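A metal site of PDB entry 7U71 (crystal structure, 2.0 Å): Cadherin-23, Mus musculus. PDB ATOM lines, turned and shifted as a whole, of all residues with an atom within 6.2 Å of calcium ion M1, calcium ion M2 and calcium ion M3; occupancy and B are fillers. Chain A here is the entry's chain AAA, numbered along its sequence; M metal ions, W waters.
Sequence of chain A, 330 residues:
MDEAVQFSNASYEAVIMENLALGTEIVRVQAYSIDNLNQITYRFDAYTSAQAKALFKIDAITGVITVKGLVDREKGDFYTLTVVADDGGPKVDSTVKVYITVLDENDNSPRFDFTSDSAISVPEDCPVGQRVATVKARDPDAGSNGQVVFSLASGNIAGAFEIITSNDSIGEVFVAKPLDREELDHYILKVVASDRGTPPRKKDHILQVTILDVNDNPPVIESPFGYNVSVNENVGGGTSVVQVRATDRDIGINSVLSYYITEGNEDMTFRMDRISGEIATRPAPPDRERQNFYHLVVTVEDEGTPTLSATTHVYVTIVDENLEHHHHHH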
ATOM      1  N   GLU A 124      13.886 -18.748 -17.212  1.00  0.00           N
ATOM      2  CA  GLU A 124      12.581 -19.062 -17.830  1.00  0.00           C
ATOM      3  C   GLU A 124      12.820 -19.907 -19.084  1.00  0.00           C
ATOM      4  O   GLU A 124      11.862 -20.519 -19.542  1.00  0.00           O
ATOM      5  CB  GLU A 124      11.796 -17.770 -18.127  1.00  0.00           C
ATOM      6  CG  GLU A 124      12.507 -16.746 -18.988  1.00  0.00           C
ATOM      7  CD  GLU A 124      11.597 -15.668 -19.560  1.00  0.00           C
ATOM      8  OE1 GLU A 124      10.384 -15.968 -19.854  1.00  0.00           O
ATOM      9  OE2 GLU A 124      12.097 -14.534 -19.741  1.00  0.00           O
ATOM     10  N   LEU A 179       8.471 -22.725 -19.116  1.00  0.00           N
ATOM     11  CA  LEU A 179       8.273 -21.596 -18.194  1.00  0.00           C
ATOM     12  C   LEU A 179       8.180 -20.311 -18.997  1.00  0.00           C
ATOM     13  O   LEU A 179       8.647 -20.266 -20.131  1.00  0.00           O
ATOM     14  CB  LEU A 179       9.395 -21.547 -17.156  1.00  0.00           C
ATOM     15  CG  LEU A 179       9.697 -22.871 -16.453  1.00  0.00           C
ATOM     16  CD1 LEU A 179      10.981 -22.780 -15.661  1.00  0.00           C
ATOM     17  CD2 LEU A 179       8.542 -23.313 -15.579  1.00  0.00           C
ATOM     18  N   ASP A 180       7.652 -19.263 -18.361  1.00  0.00           N
ATOM     19  CA  ASP A 180       7.570 -17.925 -18.977  1.00  0.00           C
ATOM     20  C   ASP A 180       7.498 -16.918 -17.839  1.00  0.00           C
ATOM     21  O   ASP A 180       6.379 -16.760 -17.290  1.00  0.00           O
ATOM     22  CB  ASP A 180       6.337 -17.835 -19.892  1.00  0.00           C
ATOM     23  CG  ASP A 180       6.224 -16.461 -20.526  1.00  0.00           C
ATOM     24  OD1 ASP A 180       7.207 -15.661 -20.479  1.00  0.00           O
ATOM     25  OD2 ASP A 180       5.176 -16.206 -21.108  1.00  0.00           O
ATOM     26  N   ARG A 181       8.596 -16.200 -17.562  1.00  0.00           N
ATOM     27  CA  ARG A 181       8.657 -15.166 -16.491  1.00  0.00           C
ATOM     28  C   ARG A 181       7.585 -14.089 -16.727  1.00  0.00           C
ATOM     29  O   ARG A 181       7.044 -13.560 -15.721  1.00  0.00           O
ATOM     30  CB  ARG A 181      10.025 -14.496 -16.431  1.00  0.00           C
ATOM     31  CG  ARG A 181      10.238 -13.589 -15.219  1.00  0.00           C
ATOM     32  CD  ARG A 181      11.152 -12.410 -15.454  1.00  0.00           C
ATOM     33  NE  ARG A 181      10.565 -11.531 -16.441  1.00  0.00           N
ATOM     34  CZ  ARG A 181       9.567 -10.667 -16.234  1.00  0.00           C
ATOM     35  NH1 ARG A 181       9.071 -10.475 -15.027  1.00  0.00           N
ATOM     36  NH2 ARG A 181       9.084 -10.001 -17.264  1.00  0.00           N
ATOM     37  N   GLU A 182       7.279 -13.781 -17.985  1.00  0.00           N
ATOM     38  CA  GLU A 182       6.271 -12.719 -18.334  1.00  0.00           C
ATOM     39  C   GLU A 182       4.849 -13.180 -17.967  1.00  0.00           C
ATOM     40  O   GLU A 182       3.969 -12.314 -17.896  1.00  0.00           O
ATOM     41  CB  GLU A 182       6.337 -12.352 -19.820  1.00  0.00           C
ATOM     42  CG  GLU A 182       7.469 -11.404 -20.133  1.00  0.00           C
ATOM     43  CD  GLU A 182       8.879 -11.965 -20.114  1.00  0.00           C
ATOM     44  OE1 GLU A 182       9.748 -11.326 -19.502  1.00  0.00           O
ATOM     45  OE2 GLU A 182       9.086 -13.082 -20.675  1.00  0.00           O
ATOM     46  N   GLU A 183       4.610 -14.478 -17.772  1.00  0.00           N
ATOM     47  CA  GLU A 183       3.305 -15.014 -17.321  1.00  0.00           C
ATOM     48  C   GLU A 183       3.364 -15.194 -15.801  1.00  0.00           C
ATOM     49  O   GLU A 183       2.464 -14.683 -15.123  1.00  0.00           O
ATOM     50  CB  GLU A 183       2.886 -16.252 -18.116  1.00  0.00           C
ATOM     51  CG  GLU A 183       1.634 -16.927 -17.555  1.00  0.00           C
ATOM     52  CD  GLU A 183       0.347 -16.104 -17.477  1.00  0.00           C
ATOM     53  OE1 GLU A 183       0.157 -15.235 -18.352  1.00  0.00           O
ATOM     54  OE2 GLU A 183      -0.476 -16.334 -16.515  1.00  0.00           O
ATOM     55  N   LEU A 212      13.962 -16.509 -13.402  1.00  0.00           N
ATOM     56  CA  LEU A 212      14.859 -15.439 -13.911  1.00  0.00           C
ATOM     57  C   LEU A 212      14.526 -15.086 -15.349  1.00  0.00           C
ATOM     58  O   LEU A 212      14.151 -15.983 -16.165  1.00  0.00           O
ATOM     59  CB  LEU A 212      16.327 -15.851 -13.768  1.00  0.00           C
ATOM     60  CG  LEU A 212      16.650 -16.345 -12.357  1.00  0.00           C
ATOM     61  CD1 LEU A 212      17.958 -17.097 -12.338  1.00  0.00           C
ATOM     62  CD2 LEU A 212      16.614 -15.171 -11.391  1.00  0.00           C
ATOM     63  N   ASP A 213      14.731 -13.799 -15.659  1.00  0.00           N
ATOM     64  CA  ASP A 213      14.375 -13.265 -16.993  1.00  0.00           C
ATOM     65  C   ASP A 213      15.384 -13.718 -18.033  1.00  0.00           C
ATOM     66  O   ASP A 213      16.565 -13.728 -17.763  1.00  0.00           O
ATOM     67  CB  ASP A 213      14.279 -11.738 -16.973  1.00  0.00           C
ATOM     68  CG  ASP A 213      13.617 -11.155 -18.202  1.00  0.00           C
ATOM     69  OD1 ASP A 213      12.573 -11.703 -18.621  1.00  0.00           O
ATOM     70  OD2 ASP A 213      14.189 -10.149 -18.736  1.00  0.00           O
ATOM     71  N   VAL A 214      14.884 -14.022 -19.221  1.00  0.00           N
ATOM     72  CA  VAL A 214      15.675 -14.140 -20.468  1.00  0.00           C
ATOM     73  C   VAL A 214      15.182 -13.025 -21.395  1.00  0.00           C
ATOM     74  O   VAL A 214      13.996 -12.634 -21.309  1.00  0.00           O
ATOM     75  CB  VAL A 214      15.479 -15.545 -21.063  1.00  0.00           C
ATOM     76  CG1 VAL A 214      16.046 -15.627 -22.465  1.00  0.00           C
ATOM     77  CG2 VAL A 214      16.116 -16.585 -20.111  1.00  0.00           C
ATOM     78  N   ASN A 215      16.071 -12.536 -22.275  1.00  0.00           N
ATOM     79  CA  ASN A 215      15.697 -11.511 -23.274  1.00  0.00           C
ATOM     80  C   ASN A 215      14.942 -12.201 -24.392  1.00  0.00           C
ATOM     81  O   ASN A 215      15.543 -12.507 -25.436  1.00  0.00           O
ATOM     82  CB  ASN A 215      16.893 -10.754 -23.839  1.00  0.00           C
ATOM     83  CG  ASN A 215      16.434  -9.502 -24.550  1.00  0.00           C
ATOM     84  OD1 ASN A 215      15.368  -8.941 -24.233  1.00  0.00           O
ATOM     85  ND2 ASN A 215      17.209  -9.064 -25.532  1.00  0.00           N
ATOM     86  N   ASP A 216      13.637 -12.396 -24.223  1.00  0.00           N
ATOM     87  CA  ASP A 216      12.865 -13.151 -25.237  1.00  0.00           C
ATOM     88  C   ASP A 216      11.697 -12.320 -25.789  1.00  0.00           C
ATOM     89  O   ASP A 216      10.883 -12.931 -26.477  1.00  0.00           O
ATOM     90  CB  ASP A 216      12.437 -14.498 -24.652  1.00  0.00           C
ATOM     91  CG  ASP A 216      11.578 -14.463 -23.388  1.00  0.00           C
ATOM     92  OD1 ASP A 216      11.400 -13.406 -22.802  1.00  0.00           O
ATOM     93  OD2 ASP A 216      11.033 -15.504 -23.072  1.00  0.00           O
ATOM     94  N   ASN A 217      11.639 -11.017 -25.482  1.00  0.00           N
ATOM     95  CA  ASN A 217      10.649 -10.063 -26.051  1.00  0.00           C
ATOM     96  C   ASN A 217      11.358  -8.894 -26.731  1.00  0.00           C
ATOM     97  O   ASN A 217      12.257  -8.254 -26.146  1.00  0.00           O
ATOM     98  CB  ASN A 217       9.658  -9.519 -25.028  1.00  0.00           C
ATOM     99  CG  ASN A 217       8.784 -10.610 -24.469  1.00  0.00           C
ATOM    100  OD1 ASN A 217       7.722 -10.894 -24.997  1.00  0.00           O
ATOM    101  ND2 ASN A 217       9.266 -11.296 -23.449  1.00  0.00           N
ATOM    102  N   PRO A 218      11.012  -8.637 -28.011  1.00  0.00           N
ATOM    103  CA  PRO A 218      11.583  -7.540 -28.762  1.00  0.00           C
ATOM    104  C   PRO A 218      10.938  -6.226 -28.332  1.00  0.00           C
ATOM    105  O   PRO A 218       9.822  -6.177 -27.816  1.00  0.00           O
ATOM    106  CB  PRO A 218      11.246  -7.901 -30.209  1.00  0.00           C
ATOM    107  CG  PRO A 218       9.916  -8.627 -30.113  1.00  0.00           C
ATOM    108  CD  PRO A 218      10.013  -9.373 -28.788  1.00  0.00           C
ATOM    109  N   PRO A 219      11.585  -5.099 -28.628  1.00  0.00           N
ATOM    110  CA  PRO A 219      10.909  -3.813 -28.564  1.00  0.00           C
ATOM    111  C   PRO A 219       9.691  -3.878 -29.490  1.00  0.00           C
ATOM    112  O   PRO A 219       9.723  -4.539 -30.493  1.00  0.00           O
ATOM    113  CB  PRO A 219      11.944  -2.786 -29.041  1.00  0.00           C
ATOM    114  CG  PRO A 219      13.256  -3.495 -29.019  1.00  0.00           C
ATOM    115  CD  PRO A 219      12.960  -4.986 -29.134  1.00  0.00           C
ATOM    116  N   ASP A 248       8.793  -2.921 -24.049  1.00  0.00           N
ATOM    117  CA  ASP A 248       9.484  -4.230 -24.059  1.00  0.00           C
ATOM    118  C   ASP A 248       9.024  -4.981 -22.819  1.00  0.00           C
ATOM    119  O   ASP A 248       9.126  -4.447 -21.725  1.00  0.00           O
ATOM    120  CB  ASP A 248      10.978  -4.020 -24.171  1.00  0.00           C
ATOM    121  CG  ASP A 248      11.787  -5.287 -24.380  1.00  0.00           C
ATOM    122  OD1 ASP A 248      11.507  -6.268 -23.661  1.00  0.00           O
ATOM    123  OD2 ASP A 248      12.778  -5.204 -25.165  1.00  0.00           O
ATOM    124  N   ARG A 249       8.551  -6.202 -23.006  1.00  0.00           N
ATOM    125  CA  ARG A 249       7.923  -6.997 -21.934  1.00  0.00           C
ATOM    126  C   ARG A 249       8.944  -7.597 -20.960  1.00  0.00           C
ATOM    127  O   ARG A 249       8.499  -8.168 -19.939  1.00  0.00           O
ATOM    128  CB  ARG A 249       7.082  -8.102 -22.588  1.00  0.00           C
ATOM    129  CG  ARG A 249       5.795  -7.577 -23.227  1.00  0.00           C
ATOM    130  CD  ARG A 249       4.943  -8.680 -23.822  1.00  0.00           C
ATOM    131  NE  ARG A 249       4.174  -9.449 -22.850  1.00  0.00           N
ATOM    132  CZ  ARG A 249       4.260 -10.767 -22.642  1.00  0.00           C
ATOM    133  NH1 ARG A 249       5.170 -11.503 -23.269  1.00  0.00           N
ATOM    134  NH2 ARG A 249       3.436 -11.332 -21.780  1.00  0.00           N
ATOM    135  N   ASP A 250      10.245  -7.520 -21.235  1.00  0.00           N
ATOM    136  CA  ASP A 250      11.254  -8.156 -20.351  1.00  0.00           C
ATOM    137  C   ASP A 250      11.498  -7.190 -19.203  1.00  0.00           C
ATOM    138  O   ASP A 250      10.732  -6.250 -19.079  1.00  0.00           O
ATOM    139  CB  ASP A 250      12.525  -8.539 -21.120  1.00  0.00           C
ATOM    140  CG  ASP A 250      12.242  -9.487 -22.266  1.00  0.00           C
ATOM    141  OD1 ASP A 250      11.617 -10.543 -22.026  1.00  0.00           O
ATOM    142  OD2 ASP A 250      12.642  -9.179 -23.375  1.00  0.00           O
ATOM    143  N   ILE A 251      12.538  -7.404 -18.390  1.00  0.00           N
ATOM    144  CA  ILE A 251      12.831  -6.539 -17.219  1.00  0.00           C
ATOM    145  C   ILE A 251      14.323  -6.210 -17.197  1.00  0.00           C
ATOM    146  O   ILE A 251      15.088  -6.912 -17.928  1.00  0.00           O
ATOM    147  CB  ILE A 251      12.366  -7.221 -15.925  1.00  0.00           C
ATOM    148  CG1 ILE A 251      13.029  -8.599 -15.737  1.00  0.00           C
ATOM    149  CG2 ILE A 251      10.849  -7.267 -15.888  1.00  0.00           C
ATOM    150  CD1 ILE A 251      12.856  -9.176 -14.343  1.00  0.00           C
ATOM    151  N   ILE A 253      17.936  -4.900 -17.852  1.00  0.00           N
ATOM    152  CA  ILE A 253      18.614  -4.491 -19.114  1.00  0.00           C
ATOM    153  C   ILE A 253      17.918  -5.091 -20.337  1.00  0.00           C
ATOM    154  O   ILE A 253      18.099  -4.511 -21.431  1.00  0.00           O
ATOM    155  CB  ILE A 253      20.135  -4.811 -19.199  1.00  0.00           C
ATOM    156  CG1 ILE A 253      20.505  -6.175 -18.630  1.00  0.00           C
ATOM    157  CG2 ILE A 253      20.967  -3.685 -18.588  1.00  0.00           C
ATOM    158  CD1 ILE A 253      19.923  -7.318 -19.365  1.00  0.00           C
ATOM    159  N   ASN A 254      17.138  -6.169 -20.178  1.00  0.00           N
ATOM    160  CA  ASN A 254      16.446  -6.821 -21.316  1.00  0.00           C
ATOM    161  C   ASN A 254      15.333  -5.888 -21.841  1.00  0.00           C
ATOM    162  O   ASN A 254      14.836  -6.145 -22.931  1.00  0.00           O
ATOM    163  CB  ASN A 254      15.902  -8.208 -20.967  1.00  0.00           C
ATOM    164  CG  ASN A 254      17.025  -9.156 -20.586  1.00  0.00           C
ATOM    165  OD1 ASN A 254      18.121  -9.103 -21.154  1.00  0.00           O
ATOM    166  ND2 ASN A 254      16.748 -10.067 -19.665  1.00  0.00           N
ATOM    167  N   SER A 255      14.959  -4.835 -21.110  1.00  0.00           N
ATOM    168  CA  SER A 255      13.912  -3.898 -21.585  1.00  0.00           C
ATOM    169  C   SER A 255      14.405  -2.460 -21.691  1.00  0.00           C
ATOM    170  O   SER A 255      13.544  -1.581 -21.835  1.00  0.00           O
ATOM    171  CB  SER A 255      12.717  -3.997 -20.711  1.00  0.00           C
ATOM    172  OG  SER A 255      13.023  -3.673 -19.385  1.00  0.00           O
ATOM    173  N   LEU A 257      15.948   0.333 -23.817  1.00  0.00           N
ATOM    174  CA  LEU A 257      15.875   0.509 -25.286  1.00  0.00           C
ATOM    175  C   LEU A 257      16.848   1.589 -25.767  1.00  0.00           C
ATOM    176  O   LEU A 257      16.983   2.622 -25.075  1.00  0.00           O
ATOM    177  CB  LEU A 257      14.442   0.881 -25.618  1.00  0.00           C
ATOM    178  CG  LEU A 257      13.434  -0.226 -25.278  1.00  0.00           C
ATOM    179  CD1 LEU A 257      12.061   0.087 -25.878  1.00  0.00           C
ATOM    180  CD2 LEU A 257      13.932  -1.567 -25.760  1.00  0.00           C
ATOM    181  N   ASP A 302      16.948  -3.429 -27.829  1.00  0.00           N
ATOM    182  CA  ASP A 302      17.064  -3.579 -26.359  1.00  0.00           C
ATOM    183  C   ASP A 302      18.533  -3.852 -26.030  1.00  0.00           C
ATOM    184  O   ASP A 302      19.301  -4.077 -26.952  1.00  0.00           O
ATOM    185  CB  ASP A 302      16.110  -4.642 -25.803  1.00  0.00           C
ATOM    186  CG  ASP A 302      16.253  -6.059 -26.341  1.00  0.00           C
ATOM    187  OD1 ASP A 302      17.344  -6.442 -26.823  1.00  0.00           O
ATOM    188  OD2 ASP A 302      15.236  -6.795 -26.248  1.00  0.00           O
ATOM    189  N   GLY A 304      19.657  -6.420 -23.961  1.00  0.00           N
ATOM    190  CA  GLY A 304      19.833  -7.826 -23.507  1.00  0.00           C
ATOM    191  C   GLY A 304      20.613  -8.687 -24.498  1.00  0.00           C
ATOM    192  O   GLY A 304      21.133  -8.144 -25.487  1.00  0.00           O
ATOM    193  N   LEU A 308      17.560  -7.870 -29.332  1.00  0.00           N
ATOM    194  CA  LEU A 308      16.328  -7.929 -30.146  1.00  0.00           C
ATOM    195  C   LEU A 308      16.003  -6.509 -30.602  1.00  0.00           C
ATOM    196  O   LEU A 308      16.301  -5.568 -29.875  1.00  0.00           O
ATOM    197  CB  LEU A 308      15.194  -8.511 -29.286  1.00  0.00           C
ATOM    198  CG  LEU A 308      15.445  -9.941 -28.817  1.00  0.00           C
ATOM    199  CD1 LEU A 308      14.271 -10.441 -27.954  1.00  0.00           C
ATOM    200  CD2 LEU A 308      15.694 -10.839 -30.016  1.00  0.00           C
HETATM  201 CA    CA M   1      13.639  -7.358 -24.589  1.00  0.00          CA
HETATM  202 CA    CA M   2      11.743 -12.427 -20.596  1.00  0.00          CA
HETATM  203 CA    CA M   3       9.137 -15.191 -21.620  1.00  0.00          CA
HETATM  204  O   HOH W   1       8.807 -17.463 -22.521  1.00  0.00           O
HETATM  205  O   HOH W   2       7.969 -14.259 -23.512  1.00  0.00           O
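The nearest printed residue that does not touch calcium ion M3 is Arg 181 (4.2 Å).
OD1 of Asp 180 is bound to calcium ion M3 (2.3 Å).
OE1 of Glu 124 is bound to calcium ion M3.
The side-chain carboxylate (OE2) of Glu 182 binds calcium ion M3, at 2.3 Å.
The side-chain carboxylate (OD2) of Asp 216 binds calcium ion M3, 2.4 Å away.
Water W2 binds calcium ion M3 (2.4 Å).
Water W1 is bound to calcium ion M3.
Calcium ion M3 has six donor atoms within binding distance.
Slightly farther from calcium ion M3 lies OD1 of Asp 216 (3.1 Å).
The side-chain amide nitrogen of Asn 217 lies close to the side-chain carboxylate of Glu 182, at 3.3 Å.
OE1 of Glu 124 sits close to N of Arg 181, 2.9 Å away.
OD1 of Asn 217 is in hydrogen-bond range of NH1 of Arg 249 (3.1 Å).
OD2 of Asp 213 lies within hydrogen-bond range of N of Ile 251.
The side-chain carboxylate (OD1) of Asp 213 lies close to the guanidinium group (NE) of Arg 181 (3.0 Å).
The backbone NH (N) of Glu 124 is in hydrogen-bond range of the backbone carbonyl oxygen (O) of Leu 212.
OE1 of Glu 182 sits close to NH2 of Arg 181, at 2.7 Å.
The backbone carbonyl oxygen (O) of Asp 250 lies close to the side-chain hydroxyl (OG) of Ser 255 (3.5 Å).
Seven residues have an atom within 4 Å of calcium ion M2: Glu 124, Glu 182, Asp 213, Val 214, Asp 216, Asn 217 and Asp 250.
Six residues have an atom within 4 Å of calcium ion M1: Asn 215, Asn 217, Asp 248, Asp 250, Asn 254 and Asp 302.
The nearest printed residue that does not touch calcium ion M1 is Ser 255 (4.5 Å).
Calcium ion M2 is bound by the side-chain carboxylate (OD1) of Asp 213 (2.3 Å), the side-chain carboxylate (OE2) of Glu 124 (2.3 Å), the side-chain carboxylate (OD1) of Asp 250 (2.4 Å), the backbone carbonyl oxygen (O) of Val 214 (2.4 Å), the side-chain carboxylate (OD1) of Asp 216 (2.4 Å), the side-chain carboxylate (OE1) of Glu 182 (2.5 Å) and the side-chain carboxylate (OE2) of Glu 182 (2.7 Å).
O of Asn 217 binds calcium ion M1 (2.3 Å).
Calcium ion M1 is bound by OD2 of Asp 302, at 2.4 Å.
OD1 of Asn 215 binds calcium ion M1, 2.4 Å away.
The backbone carbonyl oxygen (O) of Asn 254 binds calcium ion M1 (2.4 Å).
Calcium ion M1 is bound by the side-chain carboxylate (OD2) of Asp 248, 2.4 Å away.
OD2 of Asp 250 is bound to calcium ion M1, 2.4 Å away.
Calcium ion M1 is bound by OD1 of Asp 248 (2.6 Å).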
